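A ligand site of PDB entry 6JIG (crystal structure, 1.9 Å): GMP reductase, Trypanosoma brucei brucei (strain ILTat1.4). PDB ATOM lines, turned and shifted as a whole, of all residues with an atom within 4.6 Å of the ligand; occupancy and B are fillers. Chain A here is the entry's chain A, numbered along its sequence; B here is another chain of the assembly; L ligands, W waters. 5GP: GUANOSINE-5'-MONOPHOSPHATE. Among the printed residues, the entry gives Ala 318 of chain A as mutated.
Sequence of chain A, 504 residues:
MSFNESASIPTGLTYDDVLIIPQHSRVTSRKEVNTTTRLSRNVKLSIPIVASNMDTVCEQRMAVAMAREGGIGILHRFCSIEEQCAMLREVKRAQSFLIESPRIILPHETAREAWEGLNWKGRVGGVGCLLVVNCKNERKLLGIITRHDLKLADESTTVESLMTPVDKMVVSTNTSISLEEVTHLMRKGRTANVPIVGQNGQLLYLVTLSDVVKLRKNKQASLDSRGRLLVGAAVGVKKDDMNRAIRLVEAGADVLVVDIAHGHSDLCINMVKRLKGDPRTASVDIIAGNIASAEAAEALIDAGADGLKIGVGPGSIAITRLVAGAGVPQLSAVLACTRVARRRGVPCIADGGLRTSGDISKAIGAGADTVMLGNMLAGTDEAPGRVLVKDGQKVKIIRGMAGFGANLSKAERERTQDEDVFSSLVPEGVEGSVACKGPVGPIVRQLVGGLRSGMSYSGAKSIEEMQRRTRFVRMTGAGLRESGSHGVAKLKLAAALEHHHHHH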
ATOM      1  N   SER A  52      26.845  -7.235  24.889  1.00  0.00           N
ATOM      2  CA  SER A  52      25.975  -6.120  25.228  1.00  0.00           C
ATOM      3  C   SER A  52      25.042  -5.752  24.080  1.00  0.00           C
ATOM      4  O   SER A  52      25.459  -5.715  22.922  1.00  0.00           O
ATOM      5  CB  SER A  52      26.796  -4.889  25.599  1.00  0.00           C
ATOM      6  OG  SER A  52      25.955  -3.808  25.942  1.00  0.00           O
ATOM      7  N   MET A  54      24.259  -3.177  22.528  1.00  0.00           N
ATOM      8  CA  MET A  54      24.702  -1.883  22.035  1.00  0.00           C
ATOM      9  C   MET A  54      24.804  -1.951  20.523  1.00  0.00           C
ATOM     10  O   MET A  54      25.168  -2.992  19.972  1.00  0.00           O
ATOM     11  CB  MET A  54      26.059  -1.509  22.632  1.00  0.00           C
ATOM     12  CG  MET A  54      25.984  -1.259  24.127  1.00  0.00           C
ATOM     13  SD  MET A  54      27.632  -1.074  24.825  1.00  0.00           S
ATOM     14  CE  MET A  54      28.200   0.344  23.877  1.00  0.00           C
ATOM     15  N   ASN A 290      18.120  -1.492  34.255  1.00  0.00           N
ATOM     16  CA  ASN A 290      19.290  -1.787  35.078  1.00  0.00           C
ATOM     17  C   ASN A 290      19.109  -1.271  36.507  1.00  0.00           C
ATOM     18  O   ASN A 290      18.530  -0.209  36.727  1.00  0.00           O
ATOM     19  CB  ASN A 290      20.552  -1.162  34.467  1.00  0.00           C
ATOM     20  CG  ASN A 290      21.235  -2.086  33.494  1.00  0.00           C
ATOM     21  OD1 ASN A 290      20.588  -2.924  32.866  1.00  0.00           O
ATOM     22  ND2 ASN A 290      22.549  -1.973  33.386  1.00  0.00           N
ATOM     23  N   LYS A 309      19.527  -7.375  35.503  1.00  0.00           N
ATOM     24  CA  LYS A 309      20.750  -6.811  34.922  1.00  0.00           C
ATOM     25  C   LYS A 309      21.201  -5.673  35.837  1.00  0.00           C
ATOM     26  O   LYS A 309      20.445  -4.743  36.111  1.00  0.00           O
ATOM     27  CB  LYS A 309      20.533  -6.336  33.486  1.00  0.00           C
ATOM     28  CG  LYS A 309      21.873  -6.078  32.741  1.00  0.00           C
ATOM     29  CD  LYS A 309      21.835  -6.474  31.257  1.00  0.00           C
ATOM     30  CE  LYS A 309      20.926  -5.549  30.441  1.00  0.00           C
ATOM     31  NZ  LYS A 309      21.346  -4.092  30.541  1.00  0.00           N
ATOM     32  N   GLY A 313      25.609   3.241  35.583  1.00  0.00           N
ATOM     33  CA  GLY A 313      26.734   4.125  35.355  1.00  0.00           C
ATOM     34  C   GLY A 313      28.124   3.583  35.048  1.00  0.00           C
ATOM     35  O   GLY A 313      28.945   4.335  34.520  1.00  0.00           O
ATOM     36  N   PRO A 314      28.464   2.316  35.351  1.00  0.00           N
ATOM     37  CA  PRO A 314      29.874   1.915  35.241  1.00  0.00           C
ATOM     38  C   PRO A 314      30.366   1.673  33.815  1.00  0.00           C
ATOM     39  O   PRO A 314      31.566   1.410  33.626  1.00  0.00           O
ATOM     40  CB  PRO A 314      29.913   0.607  36.047  1.00  0.00           C
ATOM     41  CG  PRO A 314      28.591  -0.040  35.724  1.00  0.00           C
ATOM     42  CD  PRO A 314      27.593   1.141  35.580  1.00  0.00           C
ATOM     43  N   GLY A 315      29.483   1.764  32.817  1.00  0.00           N
ATOM     44  CA  GLY A 315      29.870   1.399  31.460  1.00  0.00           C
ATOM     45  C   GLY A 315      30.979   2.283  30.909  1.00  0.00           C
ATOM     46  O   GLY A 315      31.088   3.469  31.230  1.00  0.00           O
ATOM     47  N   SER A 316      31.825   1.680  30.057  1.00  0.00           N
ATOM     48  CA  SER A 316      32.956   2.388  29.456  1.00  0.00           C
ATOM     49  C   SER A 316      32.539   3.701  28.816  1.00  0.00           C
ATOM     50  O   SER A 316      33.226   4.716  28.954  1.00  0.00           O
ATOM     51  CB  SER A 316      33.627   1.484  28.415  1.00  0.00           C
ATOM     52  OG  SER A 316      32.742   1.226  27.332  1.00  0.00           O
ATOM     53  N   ILE A 317      31.415   3.706  28.091  1.00  0.00           N
ATOM     54  CA  ILE A 317      30.960   4.901  27.380  1.00  0.00           C
ATOM     55  C   ILE A 317      29.849   5.627  28.132  1.00  0.00           C
ATOM     56  O   ILE A 317      29.248   6.561  27.598  1.00  0.00           O
ATOM     57  CB  ILE A 317      30.542   4.555  25.925  1.00  0.00           C
ATOM     58  CG1 ILE A 317      29.452   3.475  25.882  1.00  0.00           C
ATOM     59  CG2 ILE A 317      31.719   3.960  25.168  1.00  0.00           C
ATOM     60  CD1 ILE A 317      28.209   3.796  26.617  1.00  0.00           C
ATOM     61  N   ALA A 318      29.564   5.224  29.370  1.00  0.00           N
ATOM     62  CA  ALA A 318      28.451   5.760  30.161  1.00  0.00           C
ATOM     63  C   ALA A 318      28.894   6.966  30.980  1.00  0.00           C
ATOM     64  O   ALA A 318      29.971   6.957  31.587  1.00  0.00           O
ATOM     65  CB  ALA A 318      27.914   4.685  31.102  1.00  0.00           C
ATOM     66  N   ILE A 319      28.038   7.997  31.040  1.00  0.00           N
ATOM     67  CA  ILE A 319      28.327   9.191  31.825  1.00  0.00           C
ATOM     68  C   ILE A 319      27.090   9.646  32.598  1.00  0.00           C
ATOM     69  O   ILE A 319      26.974  10.823  32.969  1.00  0.00           O
ATOM     70  CB  ILE A 319      28.852  10.337  30.938  1.00  0.00           C
ATOM     71  CG1 ILE A 319      27.869  10.652  29.817  1.00  0.00           C
ATOM     72  CG2 ILE A 319      30.241   9.999  30.385  1.00  0.00           C
ATOM     73  CD1 ILE A 319      28.238  11.890  29.024  1.00  0.00           C
ATOM     74  N   THR A 320      26.165   8.707  32.848  1.00  0.00           N
ATOM     75  CA  THR A 320      25.089   8.926  33.805  1.00  0.00           C
ATOM     76  C   THR A 320      25.599   9.520  35.122  1.00  0.00           C
ATOM     77  O   THR A 320      24.946  10.383  35.715  1.00  0.00           O
ATOM     78  CB  THR A 320      24.390   7.589  34.064  1.00  0.00           C
ATOM     79  OG1 THR A 320      23.712   7.175  32.865  1.00  0.00           O
ATOM     80  CG2 THR A 320      23.397   7.695  35.209  1.00  0.00           C
ATOM     81  N   ASP A 351      26.576  -5.968  34.553  1.00  0.00           N
ATOM     82  CA  ASP A 351      26.625  -5.251  33.273  1.00  0.00           C
ATOM     83  C   ASP A 351      27.438  -3.966  33.390  1.00  0.00           C
ATOM     84  O   ASP A 351      26.961  -2.991  33.980  1.00  0.00           O
ATOM     85  CB  ASP A 351      25.197  -4.943  32.793  1.00  0.00           C
ATOM     86  CG  ASP A 351      25.159  -4.155  31.494  1.00  0.00           C
ATOM     87  OD1 ASP A 351      26.153  -4.182  30.749  1.00  0.00           O
ATOM     88  OD2 ASP A 351      24.109  -3.525  31.230  1.00  0.00           O
ATOM     89  N   GLY A 352      28.617  -3.949  32.797  1.00  0.00           N
ATOM     90  CA  GLY A 352      29.330  -2.692  32.647  1.00  0.00           C
ATOM     91  C   GLY A 352      30.567  -2.602  33.530  1.00  0.00           C
ATOM     92  O   GLY A 352      30.608  -3.122  34.654  1.00  0.00           O
ATOM     93  N   GLY A 353      31.578  -1.889  33.035  1.00  0.00           N
ATOM     94  CA  GLY A 353      32.737  -1.575  33.841  1.00  0.00           C
ATOM     95  C   GLY A 353      33.787  -2.666  33.877  1.00  0.00           C
ATOM     96  O   GLY A 353      34.783  -2.521  34.603  1.00  0.00           O
ATOM     97  N   LEU A 354      33.609  -3.742  33.117  1.00  0.00           N
ATOM     98  CA  LEU A 354      34.584  -4.826  33.096  1.00  0.00           C
ATOM     99  C   LEU A 354      35.642  -4.533  32.050  1.00  0.00           C
ATOM    100  O   LEU A 354      35.309  -4.131  30.928  1.00  0.00           O
ATOM    101  CB  LEU A 354      33.886  -6.158  32.797  1.00  0.00           C
ATOM    102  CG  LEU A 354      32.857  -6.501  33.876  1.00  0.00           C
ATOM    103  CD1 LEU A 354      31.808  -7.431  33.310  1.00  0.00           C
ATOM    104  CD2 LEU A 354      33.536  -7.138  35.040  1.00  0.00           C
ATOM    105  N   MET A 372      28.006  -8.979  31.295  1.00  0.00           N
ATOM    106  CA  MET A 372      27.692  -8.390  30.003  1.00  0.00           C
ATOM    107  C   MET A 372      28.830  -7.461  29.610  1.00  0.00           C
ATOM    108  O   MET A 372      29.232  -6.608  30.415  1.00  0.00           O
ATOM    109  CB  MET A 372      26.363  -7.628  30.031  1.00  0.00           C
ATOM    110  CG  MET A 372      26.083  -6.917  28.715  1.00  0.00           C
ATOM    111  SD  MET A 372      24.453  -6.179  28.623  1.00  0.00           S
ATOM    112  CE  MET A 372      23.503  -7.561  27.961  1.00  0.00           C
ATOM    113  N   LEU A 373      29.333  -7.610  28.395  1.00  0.00           N
ATOM    114  CA  LEU A 373      30.505  -6.891  27.924  1.00  0.00           C
ATOM    115  C   LEU A 373      30.163  -6.038  26.720  1.00  0.00           C
ATOM    116  O   LEU A 373      29.588  -6.546  25.750  1.00  0.00           O
ATOM    117  CB  LEU A 373      31.629  -7.851  27.552  1.00  0.00           C
ATOM    118  CG  LEU A 373      32.019  -8.910  28.569  1.00  0.00           C
ATOM    119  CD1 LEU A 373      33.147  -9.748  27.996  1.00  0.00           C
ATOM    120  CD2 LEU A 373      32.469  -8.211  29.846  1.00  0.00           C
ATOM    121  N   GLY A 374      30.531  -4.762  26.778  1.00  0.00           N
ATOM    122  CA  GLY A 374      30.449  -3.905  25.610  1.00  0.00           C
ATOM    123  C   GLY A 374      31.845  -3.664  25.061  1.00  0.00           C
ATOM    124  O   GLY A 374      32.257  -4.255  24.059  1.00  0.00           O
ATOM    125  N   ASN A 375      32.598  -2.803  25.762  1.00  0.00           N
ATOM    126  CA  ASN A 375      33.910  -2.356  25.277  1.00  0.00           C
ATOM    127  C   ASN A 375      34.846  -3.514  24.943  1.00  0.00           C
ATOM    128  O   ASN A 375      35.546  -3.473  23.925  1.00  0.00           O
ATOM    129  CB  ASN A 375      34.542  -1.440  26.334  1.00  0.00           C
ATOM    130  CG  ASN A 375      35.826  -0.786  25.836  1.00  0.00           C
ATOM    131  OD1 ASN A 375      35.955  -0.466  24.657  1.00  0.00           O
ATOM    132  ND2 ASN A 375      36.756  -0.568  26.753  1.00  0.00           N
ATOM    133  N   ILE A 398      32.825   2.879  19.150  1.00  0.00           N
ATOM    134  CA  ILE A 398      31.989   2.445  20.257  1.00  0.00           C
ATOM    135  C   ILE A 398      31.271   3.681  20.795  1.00  0.00           C
ATOM    136  O   ILE A 398      31.880   4.751  20.902  1.00  0.00           O
ATOM    137  CB  ILE A 398      32.793   1.721  21.360  1.00  0.00           C
ATOM    138  CG1 ILE A 398      31.852   1.056  22.371  1.00  0.00           C
ATOM    139  CG2 ILE A 398      33.787   2.685  22.050  1.00  0.00           C
ATOM    140  CD1 ILE A 398      32.588   0.378  23.514  1.00  0.00           C
ATOM    141  N   GLY A 400      27.836   5.271  23.384  1.00  0.00           N
ATOM    142  CA  GLY A 400      26.787   5.038  24.351  1.00  0.00           C
ATOM    143  C   GLY A 400      25.411   5.092  23.717  1.00  0.00           C
ATOM    144  O   GLY A 400      25.160   5.851  22.782  1.00  0.00           O
ATOM    145  N   MET A 401      24.509   4.269  24.250  1.00  0.00           N
ATOM    146  CA  MET A 401      23.131   4.229  23.781  1.00  0.00           C
ATOM    147  C   MET A 401      22.286   5.394  24.302  1.00  0.00           C
ATOM    148  O   MET A 401      21.163   5.588  23.828  1.00  0.00           O
ATOM    149  CB  MET A 401      22.484   2.884  24.179  1.00  0.00           C
ATOM    150  CG  MET A 401      23.173   1.667  23.540  1.00  0.00           C
ATOM    151  SD  MET A 401      22.917   1.576  21.740  1.00  0.00           S
ATOM    152  CE  MET A 401      21.386   0.631  21.677  1.00  0.00           C
ATOM    153  N   ALA A 402      22.811   6.165  25.256  1.00  0.00           N
ATOM    154  CA  ALA A 402      22.195   7.426  25.666  1.00  0.00           C
ATOM    155  C   ALA A 402      22.936   8.636  25.116  1.00  0.00           C
ATOM    156  O   ALA A 402      22.663   9.764  25.533  1.00  0.00           O
ATOM    157  CB  ALA A 402      22.115   7.509  27.194  1.00  0.00           C
ATOM    158  N   GLY A 403      23.879   8.434  24.181  1.00  0.00           N
ATOM    159  CA  GLY A 403      24.600   9.513  23.553  1.00  0.00           C
ATOM    160  C   GLY A 403      23.938   9.986  22.260  1.00  0.00           C
ATOM    161  O   GLY A 403      22.923   9.443  21.808  1.00  0.00           O
ATOM    162  N   GLU A 428      23.644  10.949  28.053  1.00  0.00           N
ATOM    163  CA  GLU A 428      24.279  10.252  29.175  1.00  0.00           C
ATOM    164  C   GLU A 428      25.222   9.157  28.680  1.00  0.00           C
ATOM    165  O   GLU A 428      25.555   8.241  29.450  1.00  0.00           O
ATOM    166  CB  GLU A 428      23.228   9.688  30.133  1.00  0.00           C
ATOM    167  CG  GLU A 428      22.178  10.718  30.553  1.00  0.00           C
ATOM    168  CD  GLU A 428      21.553  10.445  31.925  1.00  0.00           C
ATOM    169  OE1 GLU A 428      21.915   9.435  32.560  1.00  0.00           O
ATOM    170  OE2 GLU A 428      20.699  11.256  32.378  1.00  0.00           O
ATOM    171  N   GLY A 429      25.658   9.251  27.422  1.00  0.00           N
ATOM    172  CA  GLY A 429      26.726   8.414  26.914  1.00  0.00           C
ATOM    173  C   GLY A 429      27.544   9.198  25.906  1.00  0.00           C
ATOM    174  O   GLY A 429      27.137  10.253  25.415  1.00  0.00           O
ATOM    175  N   HIS B 486      35.872   5.626  30.310  1.00  0.00           N
ATOM    176  CA  HIS B 486      37.112   4.887  30.467  1.00  0.00           C
ATOM    177  C   HIS B 486      37.254   3.840  29.362  1.00  0.00           C
ATOM    178  O   HIS B 486      36.272   3.200  28.974  1.00  0.00           O
ATOM    179  CB  HIS B 486      37.193   4.203  31.858  1.00  0.00           C
ATOM    180  CG  HIS B 486      35.998   3.370  32.209  1.00  0.00           C
ATOM    181  ND1 HIS B 486      35.926   2.017  31.931  1.00  0.00           N
ATOM    182  CD2 HIS B 486      34.845   3.673  32.854  1.00  0.00           C
ATOM    183  CE1 HIS B 486      34.773   1.533  32.376  1.00  0.00           C
ATOM    184  NE2 HIS B 486      34.096   2.522  32.942  1.00  0.00           N
HETATM  185  P   5GP L   1      31.221  -1.709  29.017  1.00  0.00           P
HETATM  186  O1P 5GP L   1      31.978  -1.030  30.134  1.00  0.00           O
HETATM  187  O2P 5GP L   1      31.441  -1.070  27.654  1.00  0.00           O
HETATM  188  O3P 5GP L   1      31.320  -3.215  29.015  1.00  0.00           O
HETATM  189  O5' 5GP L   1      29.707  -1.445  29.448  1.00  0.00           O
HETATM  190  C5' 5GP L   1      28.606  -1.653  28.579  1.00  0.00           C
HETATM  191  C4' 5GP L   1      27.301  -1.323  29.275  1.00  0.00           C
HETATM  192  O4' 5GP L   1      27.177   0.107  29.414  1.00  0.00           O
HETATM  193  C3' 5GP L   1      26.030  -1.707  28.530  1.00  0.00           C
HETATM  194  O3' 5GP L   1      25.708  -3.091  28.620  1.00  0.00           O
HETATM  195  C2' 5GP L   1      24.979  -0.767  29.153  1.00  0.00           C
HETATM  196  O2' 5GP L   1      24.457  -1.278  30.377  1.00  0.00           O
HETATM  197  C1' 5GP L   1      25.812   0.461  29.506  1.00  0.00           C
HETATM  198  N9  5GP L   1      25.579   1.584  28.599  1.00  0.00           N
HETATM  199  C8  5GP L   1      25.663   1.587  27.254  1.00  0.00           C
HETATM  200  N7  5GP L   1      25.390   2.847  26.818  1.00  0.00           N
HETATM  201  C5  5GP L   1      25.153   3.619  27.911  1.00  0.00           C
HETATM  202  C6  5GP L   1      24.844   4.957  28.102  1.00  0.00           C
HETATM  203  O6  5GP L   1      24.744   5.712  27.111  1.00  0.00           O
HETATM  204  N1  5GP L   1      24.654   5.418  29.344  1.00  0.00           N
HETATM  205  C2  5GP L   1      24.764   4.619  30.418  1.00  0.00           C
HETATM  206  N2  5GP L   1      24.568   5.111  31.656  1.00  0.00           N
HETATM  207  N3  5GP L   1      25.081   3.309  30.264  1.00  0.00           N
HETATM  208  C4  5GP L   1      25.280   2.808  29.024  1.00  0.00           C
HETATM  209  O   HOH W   1      33.668  -4.522  28.425  1.00  0.00           O
HETATM  210  O   HOH W   2      23.723   3.169  33.466  1.00  0.00           O
HETATM  211  O   HOH W   3      26.037  -0.660  32.752  1.00  0.00           O
HETATM  212  O   HOH W   4      31.360  -4.626  31.220  1.00  0.00           O
HETATM  213  O   HOH W   5      26.541   1.974  32.645  1.00  0.00           O
HETATM  214  O   HOH W   6      22.847  -3.094  28.123  1.00  0.00           O
HETATM  215  O   HOH W   7      34.555  -1.518  30.522  1.00  0.00           O
HETATM  216  O   HOH W   8      22.811   1.032  31.433  1.00  0.00           O
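Merely in contact with the ligand: Ile 317 (3.0 Å), Ala 318 (3.2 Å), Gly 429 (3.4 Å), Gly 352 (3.5 Å), Gly 315 (3.5 Å), Gly 400 (3.5 Å), Asn 290 (3.6 Å), Leu 373 (3.8 Å) and Met 54 (3.9 Å).
Hydrophobic or aromatic side chains within 4 Å of the ligand: Met 54, Ile 317, Ala 318, Met 372, Met 401 and Ala 402.
The nearest printed residue that does not touch the ligand is Gly 403 (4.1 Å).
Water W7 lies within hydrogen-bond range of O1P of the ligand (2.7 Å) and O of Leu 354 (2.7 Å).
Water W1 lies within hydrogen-bond range of an oxygen (O3P) of the ligand, the backbone carbonyl oxygen (O) of Leu 354 and the backbone NH (N) of Asn 375.
Water W2 bridges a nitrogen (N2) of the ligand and the backbone NH (N) of Gly 313.
Water W6 lies within hydrogen-bond range of O3' of the ligand (2.9 Å), NZ of Lys 309 (3.0 Å), OD2 of Asp 351 (3.4 Å) and SD of Met 372 (3.5 Å).
Water W3 bridges the backbone carbonyl oxygen (O) of Asp 351 and an oxygen (O2') of the ligand.
Water W5 lies within hydrogen-bond range of N of Gly 315 (3.0 Å), N3 of the ligand (3.1 Å) and N of Gly 313 (3.3 Å).
N of Ser 316 lies within hydrogen-bond range of O1P of the ligand, 2.7 Å away.
The side-chain carboxylate of Asp 351 is in hydrogen-bond range of an oxygen (O2') of the ligand, at 2.4 Å.
The backbone NH of Met 401 lies within hydrogen-bond range of a nitrogen (N7) of the ligand, 3.1 Å away.
SD of Met 372 sits at hydrogen-bond distance from O3' of the ligand, at 3.3 Å.
The backbone carbonyl oxygen (O) of Glu 428 is in hydrogen-bond range of a nitrogen (N1) of the ligand (3.0 Å).
The side-chain hydroxyl (OG1) of Thr 320 sits at hydrogen-bond distance from a nitrogen (N2) of the ligand, 2.5 Å away.
The backbone NH (N) of Asn 375 is in hydrogen-bond range of an oxygen (O2P) of the ligand (2.8 Å).
An oxygen (O3') of the ligand lies within hydrogen-bond range of the side-chain hydroxyl (OG) of Ser 52 (2.8 Å).
N of Gly 353 sits at hydrogen-bond distance from O1P of the ligand, 3.1 Å away.
O2P of the ligand is in hydrogen-bond range of OG of Ser 316, 2.7 Å away.
The backbone NH (N) of Gly 374 lies within hydrogen-bond range of an oxygen (O3P) of the ligand.
An oxygen (O6) of the ligand sits at hydrogen-bond distance from the backbone NH (N) of Ala 402 (2.7 Å).
The side-chain carboxylate (OD2) of Asp 351 is in salt-bridge range of the side-chain amino group (NZ) of Lys 309, 2.9 Å away.
The backbone NH of Ile 319 sits at hydrogen-bond distance from the backbone carbonyl oxygen of Glu 428, 3.0 Å away.
OG1 of Thr 320 lies within hydrogen-bond range of OE1 of Glu 428, 2.9 Å away.
ND2 of Asn 290 sits at hydrogen-bond distance from OD2 of Asp 351, at 3.1 Å.
The backbone NH (N) of His 486 of chain B is in hydrogen-bond range of the backbone carbonyl oxygen (O) of Ser 316 (3.1 Å).
N of Ser 52 lies within hydrogen-bond range of O of Leu 373, 3.0 Å away.
OG of Ser 52 lies close to SD of Met 54, at 3.4 Å.
NZ of Lys 309 lies within hydrogen-bond range of OD1 of Asn 290 (2.7 Å).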
